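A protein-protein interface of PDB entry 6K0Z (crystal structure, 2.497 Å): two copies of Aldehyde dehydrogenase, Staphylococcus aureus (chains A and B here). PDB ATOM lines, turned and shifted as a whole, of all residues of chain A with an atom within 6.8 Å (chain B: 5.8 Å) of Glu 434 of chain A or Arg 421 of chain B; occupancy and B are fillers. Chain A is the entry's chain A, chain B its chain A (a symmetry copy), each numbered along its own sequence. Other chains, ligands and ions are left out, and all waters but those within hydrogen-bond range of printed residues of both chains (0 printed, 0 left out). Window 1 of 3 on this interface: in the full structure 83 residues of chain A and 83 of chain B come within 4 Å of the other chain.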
ATOM      1  N   ILE A 107       0.681 -12.872  -4.570  1.00  0.00           N
ATOM      2  CA  ILE A 107       1.036 -12.174  -5.793  1.00  0.00           C
ATOM      3  C   ILE A 107       2.537 -11.947  -5.749  1.00  0.00           C
ATOM      4  O   ILE A 107       3.036 -11.231  -4.870  1.00  0.00           O
ATOM      5  CB  ILE A 107       0.292 -10.842  -5.949  1.00  0.00           C
ATOM      6  CG1 ILE A 107      -1.194 -11.096  -6.189  1.00  0.00           C
ATOM      7  CG2 ILE A 107       0.896 -10.034  -7.097  1.00  0.00           C
ATOM      8  CD1 ILE A 107      -2.045  -9.876  -6.004  1.00  0.00           C
ATOM      9  N   LYS A 108       3.255 -12.546  -6.696  1.00  0.00           N
ATOM     10  CA  LYS A 108       4.695 -12.387  -6.793  1.00  0.00           C
ATOM     11  C   LYS A 108       5.000 -11.266  -7.775  1.00  0.00           C
ATOM     12  O   LYS A 108       4.304 -11.108  -8.783  1.00  0.00           O
ATOM     13  CB  LYS A 108       5.333 -13.703  -7.232  1.00  0.00           C
ATOM     14  CG  LYS A 108       6.805 -13.610  -7.607  1.00  0.00           C
ATOM     15  CD  LYS A 108       7.468 -14.963  -7.557  1.00  0.00           C
ATOM     16  CE  LYS A 108       8.969 -14.841  -7.401  1.00  0.00           C
ATOM     17  NZ  LYS A 108       9.670 -14.679  -8.719  1.00  0.00           N
ATOM     18  N   LYS A 109       6.011 -10.465  -7.463  1.00  0.00           N
ATOM     19  CA  LYS A 109       6.389  -9.328  -8.296  1.00  0.00           C
ATOM     20  C   LYS A 109       7.650  -9.717  -9.060  1.00  0.00           C
ATOM     21  O   LYS A 109       8.754  -9.668  -8.511  1.00  0.00           O
ATOM     22  CB  LYS A 109       6.617  -8.077  -7.455  1.00  0.00           C
ATOM     23  CG  LYS A 109       5.645  -7.881  -6.282  1.00  0.00           C
ATOM     24  CD  LYS A 109       4.353  -7.224  -6.717  1.00  0.00           C
ATOM     25  CE  LYS A 109       3.581  -6.696  -5.526  1.00  0.00           C
ATOM     26  NZ  LYS A 109       3.810  -5.230  -5.340  1.00  0.00           N
ATOM     27  N   GLU A 110       7.493 -10.080 -10.335  1.00  0.00           N
ATOM     28  CA  GLU A 110       8.597 -10.602 -11.131  1.00  0.00           C
ATOM     29  C   GLU A 110       8.879  -9.721 -12.348  1.00  0.00           C
ATOM     30  O   GLU A 110       7.975  -9.056 -12.873  1.00  0.00           O
ATOM     31  CB  GLU A 110       8.308 -12.040 -11.585  1.00  0.00           C
ATOM     32  CG  GLU A 110       7.531 -12.143 -12.879  1.00  0.00           C
ATOM     33  CD  GLU A 110       7.106 -13.578 -13.191  1.00  0.00           C
ATOM     34  OE1 GLU A 110       7.450 -14.476 -12.391  1.00  0.00           O
ATOM     35  OE2 GLU A 110       6.491 -13.813 -14.261  1.00  0.00           O
ATOM     36  N   TYR A 112       9.871  -8.468 -16.245  1.00  0.00           N
ATOM     37  CA  TYR A 112       9.469  -8.874 -17.583  1.00  0.00           C
ATOM     38  C   TYR A 112      10.592  -9.597 -18.303  1.00  0.00           C
ATOM     39  O   TYR A 112      10.338 -10.546 -19.052  1.00  0.00           O
ATOM     40  CB  TYR A 112       9.029  -7.660 -18.399  1.00  0.00           C
ATOM     41  CG  TYR A 112       7.596  -7.262 -18.163  1.00  0.00           C
ATOM     42  CD1 TYR A 112       6.552  -7.968 -18.755  1.00  0.00           C
ATOM     43  CD2 TYR A 112       7.282  -6.178 -17.348  1.00  0.00           C
ATOM     44  CE1 TYR A 112       5.234  -7.603 -18.540  1.00  0.00           C
ATOM     45  CE2 TYR A 112       5.976  -5.809 -17.124  1.00  0.00           C
ATOM     46  CZ  TYR A 112       4.958  -6.520 -17.715  1.00  0.00           C
ATOM     47  OH  TYR A 112       3.664  -6.136 -17.471  1.00  0.00           O
ATOM     48  N   ARG A 421       2.212   4.791 -17.100  1.00  0.00           N
ATOM     49  CA  ARG A 421       2.633   5.819 -16.150  1.00  0.00           C
ATOM     50  C   ARG A 421       3.851   5.337 -15.375  1.00  0.00           C
ATOM     51  O   ARG A 421       4.119   4.136 -15.299  1.00  0.00           O
ATOM     52  CB  ARG A 421       1.508   6.165 -15.178  1.00  0.00           C
ATOM     53  CG  ARG A 421       1.122   4.995 -14.315  1.00  0.00           C
ATOM     54  CD  ARG A 421      -0.368   4.790 -14.345  1.00  0.00           C
ATOM     55  NE  ARG A 421      -0.760   3.511 -13.750  1.00  0.00           N
ATOM     56  CZ  ARG A 421      -1.294   3.378 -12.543  1.00  0.00           C
ATOM     57  NH1 ARG A 421      -1.623   2.177 -12.089  1.00  0.00           N
ATOM     58  NH2 ARG A 421      -1.509   4.445 -11.794  1.00  0.00           N
ATOM     59  N   LYS A 425       7.019   4.445  -7.129  1.00  0.00           N
ATOM     60  CA  LYS A 425       6.668   3.041  -7.271  1.00  0.00           C
ATOM     61  C   LYS A 425       6.170   2.739  -8.680  1.00  0.00           C
ATOM     62  O   LYS A 425       6.515   1.698  -9.240  1.00  0.00           O
ATOM     63  CB  LYS A 425       5.633   2.644  -6.219  1.00  0.00           C
ATOM     64  CG  LYS A 425       5.461   1.140  -6.057  1.00  0.00           C
ATOM     65  CD  LYS A 425       4.236   0.790  -5.217  1.00  0.00           C
ATOM     66  CE  LYS A 425       4.191  -0.712  -4.884  1.00  0.00           C
ATOM     67  NZ  LYS A 425       3.369  -1.480  -5.876  1.00  0.00           N
ATOM     68  N   PHE A 428       8.571   1.278 -10.887  1.00  0.00           N
ATOM     69  CA  PHE A 428       8.765  -0.132 -10.571  1.00  0.00           C
ATOM     70  C   PHE A 428       7.652  -0.994 -11.165  1.00  0.00           C
ATOM     71  O   PHE A 428       7.923  -2.038 -11.769  1.00  0.00           O
ATOM     72  CB  PHE A 428       8.849  -0.304  -9.050  1.00  0.00           C
ATOM     73  CG  PHE A 428       8.780  -1.729  -8.598  1.00  0.00           C
ATOM     74  CD1 PHE A 428       9.922  -2.510  -8.543  1.00  0.00           C
ATOM     75  CD2 PHE A 428       7.569  -2.290  -8.232  1.00  0.00           C
ATOM     76  CE1 PHE A 428       9.852  -3.831  -8.134  1.00  0.00           C
ATOM     77  CE2 PHE A 428       7.487  -3.601  -7.835  1.00  0.00           C
ATOM     78  CZ  PHE A 428       8.627  -4.378  -7.779  1.00  0.00           C
ATOM     79  N   ASP A 429       6.392  -0.572 -10.990  1.00  0.00           N
ATOM     80  CA  ASP A 429       5.246  -1.355 -11.450  1.00  0.00           C
ATOM     81  C   ASP A 429       5.206  -1.465 -12.970  1.00  0.00           C
ATOM     82  O   ASP A 429       4.804  -2.501 -13.510  1.00  0.00           O
ATOM     83  CB  ASP A 429       3.938  -0.746 -10.928  1.00  0.00           C
ATOM     84  CG  ASP A 429       3.875  -0.693  -9.394  1.00  0.00           C
ATOM     85  OD1 ASP A 429       4.927  -0.457  -8.744  1.00  0.00           O
ATOM     86  OD2 ASP A 429       2.764  -0.897  -8.848  1.00  0.00           O
ATOM     87  N   THR A 432       7.068  -4.486 -13.940  1.00  0.00           N
ATOM     88  CA  THR A 432       6.806  -5.663 -13.125  1.00  0.00           C
ATOM     89  C   THR A 432       5.641  -6.448 -13.699  1.00  0.00           C
ATOM     90  O   THR A 432       4.661  -5.861 -14.160  1.00  0.00           O
ATOM     91  CB  THR A 432       6.473  -5.279 -11.684  1.00  0.00           C
ATOM     92  OG1 THR A 432       7.614  -4.661 -11.081  1.00  0.00           O
ATOM     93  CG2 THR A 432       6.065  -6.505 -10.878  1.00  0.00           C
ATOM     94  N   HIS A 433       5.739  -7.769 -13.665  1.00  0.00           N
ATOM     95  CA  HIS A 433       4.567  -8.606 -13.851  1.00  0.00           C
ATOM     96  C   HIS A 433       4.096  -9.061 -12.478  1.00  0.00           C
ATOM     97  O   HIS A 433       4.895  -9.552 -11.670  1.00  0.00           O
ATOM     98  CB  HIS A 433       4.859  -9.804 -14.757  1.00  0.00           C
ATOM     99  CG  HIS A 433       3.718 -10.768 -14.858  1.00  0.00           C
ATOM    100  ND1 HIS A 433       2.427 -10.371 -15.144  1.00  0.00           N
ATOM    101  CD2 HIS A 433       3.665 -12.107 -14.671  1.00  0.00           C
ATOM    102  CE1 HIS A 433       1.633 -11.427 -15.144  1.00  0.00           C
ATOM    103  NE2 HIS A 433       2.360 -12.493 -14.858  1.00  0.00           N
ATOM    104  N   GLU A 434       2.817  -8.855 -12.194  1.00  0.00           N
ATOM    105  CA  GLU A 434       2.236  -9.331 -10.948  1.00  0.00           C
ATOM    106  C   GLU A 434       1.652 -10.706 -11.220  1.00  0.00           C
ATOM    107  O   GLU A 434       0.727 -10.848 -12.024  1.00  0.00           O
ATOM    108  CB  GLU A 434       1.194  -8.357 -10.414  1.00  0.00           C
ATOM    109  CG  GLU A 434       1.827  -7.105  -9.892  1.00  0.00           C
ATOM    110  CD  GLU A 434       0.869  -6.257  -9.107  1.00  0.00           C
ATOM    111  OE1 GLU A 434      -0.363  -6.472  -9.217  1.00  0.00           O
ATOM    112  OE2 GLU A 434       1.359  -5.378  -8.371  1.00  0.00           O
ATOM    113  N   LYS A 435       2.221 -11.717 -10.580  1.00  0.00           N
ATOM    114  CA  LYS A 435       1.926 -13.110 -10.879  1.00  0.00           C
ATOM    115  C   LYS A 435       1.146 -13.694  -9.707  1.00  0.00           C
ATOM    116  O   LYS A 435       1.707 -13.935  -8.633  1.00  0.00           O
ATOM    117  CB  LYS A 435       3.219 -13.885 -11.142  1.00  0.00           C
ATOM    118  CG  LYS A 435       3.023 -15.276 -11.732  1.00  0.00           C
ATOM    119  CD  LYS A 435       4.357 -15.905 -12.158  1.00  0.00           C
ATOM    120  CE  LYS A 435       5.087 -16.518 -10.975  1.00  0.00           C
ATOM    121  NZ  LYS A 435       6.522 -16.759 -11.295  1.00  0.00           N
ATOM    122  N   SER A 436      -0.146 -13.910  -9.914  1.00  0.00           N
ATOM    123  CA  SER A 436      -0.978 -14.539  -8.903  1.00  0.00           C
ATOM    124  C   SER A 436      -0.683 -16.030  -8.840  1.00  0.00           C
ATOM    125  O   SER A 436      -0.729 -16.722  -9.856  1.00  0.00           O
ATOM    126  CB  SER A 436      -2.454 -14.326  -9.219  1.00  0.00           C
ATOM    127  OG  SER A 436      -2.769 -12.955  -9.251  1.00  0.00           O
ATOM    128  N   PHE B 192     -10.834  -4.451 -24.836  1.00  0.00           N
ATOM    129  CA  PHE B 192     -10.627  -5.615 -23.989  1.00  0.00           C
ATOM    130  C   PHE B 192     -10.911  -6.863 -24.813  1.00  0.00           C
ATOM    131  O   PHE B 192     -12.002  -7.000 -25.381  1.00  0.00           O
ATOM    132  CB  PHE B 192     -11.533  -5.556 -22.756  1.00  0.00           C
ATOM    133  CG  PHE B 192     -11.255  -6.623 -21.738  1.00  0.00           C
ATOM    134  CD1 PHE B 192     -11.735  -7.918 -21.910  1.00  0.00           C
ATOM    135  CD2 PHE B 192     -10.531  -6.328 -20.591  1.00  0.00           C
ATOM    136  CE1 PHE B 192     -11.484  -8.896 -20.967  1.00  0.00           C
ATOM    137  CE2 PHE B 192     -10.287  -7.300 -19.645  1.00  0.00           C
ATOM    138  CZ  PHE B 192     -10.766  -8.588 -19.835  1.00  0.00           C
ATOM    139  N   THR B 215      -6.203  -4.579 -23.262  1.00  0.00           N
ATOM    140  CA  THR B 215      -5.924  -5.766 -22.468  1.00  0.00           C
ATOM    141  C   THR B 215      -6.182  -6.976 -23.351  1.00  0.00           C
ATOM    142  O   THR B 215      -7.303  -7.175 -23.826  1.00  0.00           O
ATOM    143  CB  THR B 215      -6.795  -5.823 -21.208  1.00  0.00           C
ATOM    144  OG1 THR B 215      -6.393  -4.790 -20.303  1.00  0.00           O
ATOM    145  CG2 THR B 215      -6.653  -7.161 -20.510  1.00  0.00           C
ATOM    146  N   GLU B 217      -5.990 -11.151 -23.532  1.00  0.00           N
ATOM    147  CA  GLU B 217      -5.906 -12.386 -22.756  1.00  0.00           C
ATOM    148  C   GLU B 217      -6.003 -13.543 -23.736  1.00  0.00           C
ATOM    149  O   GLU B 217      -7.108 -13.927 -24.142  1.00  0.00           O
ATOM    150  CB  GLU B 217      -6.991 -12.463 -21.710  1.00  0.00           C
ATOM    151  CG  GLU B 217      -6.927 -11.277 -20.816  1.00  0.00           C
ATOM    152  CD  GLU B 217      -7.096 -11.668 -19.387  1.00  0.00           C
ATOM    153  OE1 GLU B 217      -7.368 -12.866 -19.135  1.00  0.00           O
ATOM    154  OE2 GLU B 217      -6.928 -10.784 -18.526  1.00  0.00           O
ATOM    155  N   GLY B 393       1.553 -16.418 -16.498  1.00  0.00           N
ATOM    156  CA  GLY B 393       0.458 -15.526 -16.164  1.00  0.00           C
ATOM    157  C   GLY B 393       0.137 -15.585 -14.688  1.00  0.00           C
ATOM    158  O   GLY B 393       0.487 -14.666 -13.943  1.00  0.00           O
ATOM    159  N   PRO B 410      -5.353 -10.831  -9.359  1.00  0.00           N
ATOM    160  CA  PRO B 410      -5.458 -10.446 -10.772  1.00  0.00           C
ATOM    161  C   PRO B 410      -5.314 -11.660 -11.669  1.00  0.00           C
ATOM    162  O   PRO B 410      -4.546 -12.581 -11.379  1.00  0.00           O
ATOM    163  CB  PRO B 410      -4.290  -9.474 -10.956  1.00  0.00           C
ATOM    164  CG  PRO B 410      -3.315  -9.846  -9.889  1.00  0.00           C
ATOM    165  CD  PRO B 410      -4.166 -10.253  -8.713  1.00  0.00           C
ATOM    166  N   PHE B 411      -6.084 -11.661 -12.751  1.00  0.00           N
ATOM    167  CA  PHE B 411      -6.057 -12.725 -13.741  1.00  0.00           C
ATOM    168  C   PHE B 411      -5.628 -12.126 -15.071  1.00  0.00           C
ATOM    169  O   PHE B 411      -6.339 -11.285 -15.630  1.00  0.00           O
ATOM    170  CB  PHE B 411      -7.421 -13.409 -13.863  1.00  0.00           C
ATOM    171  CG  PHE B 411      -7.484 -14.419 -14.966  1.00  0.00           C
ATOM    172  CD1 PHE B 411      -6.481 -15.367 -15.104  1.00  0.00           C
ATOM    173  CD2 PHE B 411      -8.535 -14.418 -15.878  1.00  0.00           C
ATOM    174  CE1 PHE B 411      -6.518 -16.296 -16.124  1.00  0.00           C
ATOM    175  CE2 PHE B 411      -8.582 -15.351 -16.906  1.00  0.00           C
ATOM    176  CZ  PHE B 411      -7.568 -16.291 -17.025  1.00  0.00           C
ATOM    177  N   GLY B 412      -4.468 -12.545 -15.560  1.00  0.00           N
ATOM    178  CA  GLY B 412      -3.969 -12.052 -16.830  1.00  0.00           C
ATOM    179  C   GLY B 412      -2.685 -12.761 -17.199  1.00  0.00           C
ATOM    180  O   GLY B 412      -2.025 -13.388 -16.364  1.00  0.00           O
ATOM    181  N   MET B 419      -1.476  -9.496 -21.970  1.00  0.00           N
ATOM    182  CA  MET B 419      -1.053  -8.296 -21.267  1.00  0.00           C
ATOM    183  C   MET B 419      -2.272  -7.675 -20.602  1.00  0.00           C
ATOM    184  O   MET B 419      -3.372  -7.699 -21.162  1.00  0.00           O
ATOM    185  CB  MET B 419      -0.388  -7.287 -22.213  1.00  0.00           C
ATOM    186  CG  MET B 419      -1.259  -6.868 -23.382  1.00  0.00           C
ATOM    187  SD  MET B 419      -0.452  -5.654 -24.444  1.00  0.00           S
ATOM    188  CE  MET B 419       0.888  -6.645 -25.088  1.00  0.00           C
ATOM    189  N   GLY B 420      -2.081  -7.131 -19.409  1.00  0.00           N
ATOM    190  CA  GLY B 420      -3.199  -6.623 -18.642  1.00  0.00           C
ATOM    191  C   GLY B 420      -3.805  -7.698 -17.773  1.00  0.00           C
ATOM    192  O   GLY B 420      -3.348  -8.844 -17.733  1.00  0.00           O
ATOM    193  N   ARG B 421      -4.868  -7.325 -17.061  1.00  0.00           N
ATOM    194  CA  ARG B 421      -5.466  -8.243 -16.094  1.00  0.00           C
ATOM    195  C   ARG B 421      -6.800  -7.690 -15.614  1.00  0.00           C
ATOM    196  O   ARG B 421      -7.065  -6.491 -15.724  1.00  0.00           O
ATOM    197  CB  ARG B 421      -4.541  -8.466 -14.901  1.00  0.00           C
ATOM    198  CG  ARG B 421      -4.306  -7.202 -14.119  1.00  0.00           C
ATOM    199  CD  ARG B 421      -2.833  -6.986 -13.900  1.00  0.00           C
ATOM    200  NE  ARG B 421      -2.543  -5.645 -13.392  1.00  0.00           N
ATOM    201  CZ  ARG B 421      -2.237  -5.370 -12.131  1.00  0.00           C
ATOM    202  NH1 ARG B 421      -1.983  -4.123 -11.763  1.00  0.00           N
ATOM    203  NH2 ARG B 421      -2.173  -6.344 -11.240  1.00  0.00           N
ATOM    204  N   TYR B 422      -7.623  -8.572 -15.057  1.00  0.00           N
ATOM    205  CA  TYR B 422      -8.927  -8.165 -14.531  1.00  0.00           C
ATOM    206  C   TYR B 422      -9.317  -9.119 -13.401  1.00  0.00           C
ATOM    207  O   TYR B 422      -8.454  -9.757 -12.790  1.00  0.00           O
ATOM    208  CB  TYR B 422      -9.967  -8.082 -15.669  1.00  0.00           C
ATOM    209  CG  TYR B 422     -10.331  -9.397 -16.317  1.00  0.00           C
ATOM    210  CD1 TYR B 422      -9.380 -10.140 -16.983  1.00  0.00           C
ATOM    211  CD2 TYR B 422     -11.637  -9.872 -16.297  1.00  0.00           C
ATOM    212  CE1 TYR B 422      -9.702 -11.334 -17.584  1.00  0.00           C
ATOM    213  CE2 TYR B 422     -11.971 -11.070 -16.905  1.00  0.00           C
ATOM    214  CZ  TYR B 422     -10.994 -11.791 -17.544  1.00  0.00           C
ATOM    215  OH  TYR B 422     -11.284 -12.981 -18.156  1.00  0.00           O
ATOM    216  N   HIS B 423     -10.627  -9.218 -13.142  1.00  0.00           N
ATOM    217  CA  HIS B 423     -11.245  -9.859 -11.979  1.00  0.00           C
ATOM    218  C   HIS B 423     -11.209  -8.938 -10.765  1.00  0.00           C
ATOM    219  O   HIS B 423     -10.165  -8.363 -10.439  1.00  0.00           O
ATOM    220  CB  HIS B 423     -10.594 -11.205 -11.630  1.00  0.00           C
ATOM    221  CG  HIS B 423     -10.960 -12.310 -12.565  1.00  0.00           C
ATOM    222  ND1 HIS B 423     -11.701 -12.099 -13.709  1.00  0.00           N
ATOM    223  CD2 HIS B 423     -10.722 -13.641 -12.509  1.00  0.00           C
ATOM    224  CE1 HIS B 423     -11.882 -13.251 -14.332  1.00  0.00           C
ATOM    225  NE2 HIS B 423     -11.300 -14.201 -13.622  1.00  0.00           N
ATOM    226  N   TYR B 426      -9.440  -5.355 -10.154  1.00  0.00           N
ATOM    227  CA  TYR B 426      -8.630  -5.222 -11.368  1.00  0.00           C
ATOM    228  C   TYR B 426      -9.485  -4.985 -12.608  1.00  0.00           C
ATOM    229  O   TYR B 426      -9.087  -4.234 -13.504  1.00  0.00           O
ATOM    230  CB  TYR B 426      -7.752  -6.451 -11.539  1.00  0.00           C
ATOM    231  CG  TYR B 426      -6.781  -6.580 -10.400  1.00  0.00           C
ATOM    232  CD1 TYR B 426      -5.598  -5.854 -10.389  1.00  0.00           C
ATOM    233  CD2 TYR B 426      -7.061  -7.396  -9.317  1.00  0.00           C
ATOM    234  CE1 TYR B 426      -4.716  -5.951  -9.349  1.00  0.00           C
ATOM    235  CE2 TYR B 426      -6.182  -7.500  -8.266  1.00  0.00           C
ATOM    236  CZ  TYR B 426      -5.008  -6.771  -8.289  1.00  0.00           C
ATOM    237  OH  TYR B 426      -4.103  -6.842  -7.257  1.00  0.00           O
ATOM    238  N   SER B 427     -10.675  -5.595 -12.669  1.00  0.00           N
ATOM    239  CA  SER B 427     -11.631  -5.248 -13.719  1.00  0.00           C
ATOM    240  C   SER B 427     -11.925  -3.754 -13.721  1.00  0.00           C
ATOM    241  O   SER B 427     -11.903  -3.101 -14.767  1.00  0.00           O
ATOM    242  CB  SER B 427     -12.926  -6.037 -13.536  1.00  0.00           C
ATOM    243  OG  SER B 427     -12.708  -7.413 -13.752  1.00  0.00           O
ATOM    244  N   THR B 430      -8.802  -1.798 -14.926  1.00  0.00           N
ATOM    245  CA  THR B 430      -8.548  -1.917 -16.359  1.00  0.00           C
ATOM    246  C   THR B 430      -9.253  -0.818 -17.134  1.00  0.00           C
ATOM    247  O   THR B 430      -8.689  -0.260 -18.076  1.00  0.00           O
ATOM    248  CB  THR B 430      -8.980  -3.301 -16.857  1.00  0.00           C
ATOM    249  OG1 THR B 430      -8.059  -4.285 -16.360  1.00  0.00           O
ATOM    250  CG2 THR B 430      -8.985  -3.362 -18.356  1.00  0.00           C
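The backbone carbonyl oxygen (O) of Gly 393 of chain B is in hydrogen-bond range of a ring nitrogen (NE2) of His 433 of chain A (3.0 Å). OE1 of Glu 434 of chain A lies within salt-bridge range of NH2 of Arg 421 of chain B, 2.7 Å away. OG of Ser 436 of chain A is in hydrogen-bond range of O of Pro 410 of chain B (2.8 Å).
N of Lys 435 of chain A is in hydrogen-bond range of O of Lys 108 of chain A (2.8 Å). OE2 of Glu 434 of chain A lies within salt-bridge range of NZ of Lys 109 of chain A (3.9 Å). O of Glu 110 of chain A is in hydrogen-bond range of N of His 433 of chain A, at 2.7 Å. The side-chain carboxylate (OE1) of Glu 110 of chain A is in salt-bridge range of the side-chain amino group (NZ) of Lys 435 of chain A (2.7 Å). The side-chain hydroxyl (OG1) of Thr 430 of chain B is in hydrogen-bond range of the backbone carbonyl oxygen (O) of Arg 421 of chain B (2.5 Å). O of Tyr 426 of chain B is in hydrogen-bond range of OG1 of Thr 430 of chain B (3.0 Å).
Among the printed residues, pairs that only touch across the chains: Lys 435 of chain A with Gly 393 of chain B (3.4 Å), Ile 107 of chain A with Pro 410 of chain B (3.5 Å) and Ile 107 of chain A with Tyr 426 of chain B (3.9 Å).
Of chain B, only Arg 421 comes within 4 Å of Glu 434 of chain A. Arg 421 of chain B touches just one residue of chain A: Glu 434. Printed residues of chain B within 4 Å of Lys 435 of chain A: Gly 393. Printed residues of chain A within 4 Å of Tyr 426 of chain B: Ile 107 (3.9 Å). Of the printed residues of chain B, His 433 of chain A touches Gly 393 (3.0 Å). Of the printed residues of chain B, Ser 436 of chain A touches Pro 410 (2.8 Å). Of the printed residues of chain A, Pro 410 of chain B touches Ile 107 and Ser 436. The nearest printed residue of chain A that does not touch Arg 421 of chain B is Ile 107 of chain A (6.3 Å).
Among the printed residues, 6 pairs touch across the chains. Among the printed residues, Asp or Glu carboxylates within 4 Å of a Lys or Arg side-chain nitrogen of the other chain: Glu 434 of chain A with Arg 421 of chain B.
1 position is printed for both chains. Of the 6 pairs that touch across the chains among the printed residues, none has its exchanged pair printed and touching as well.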
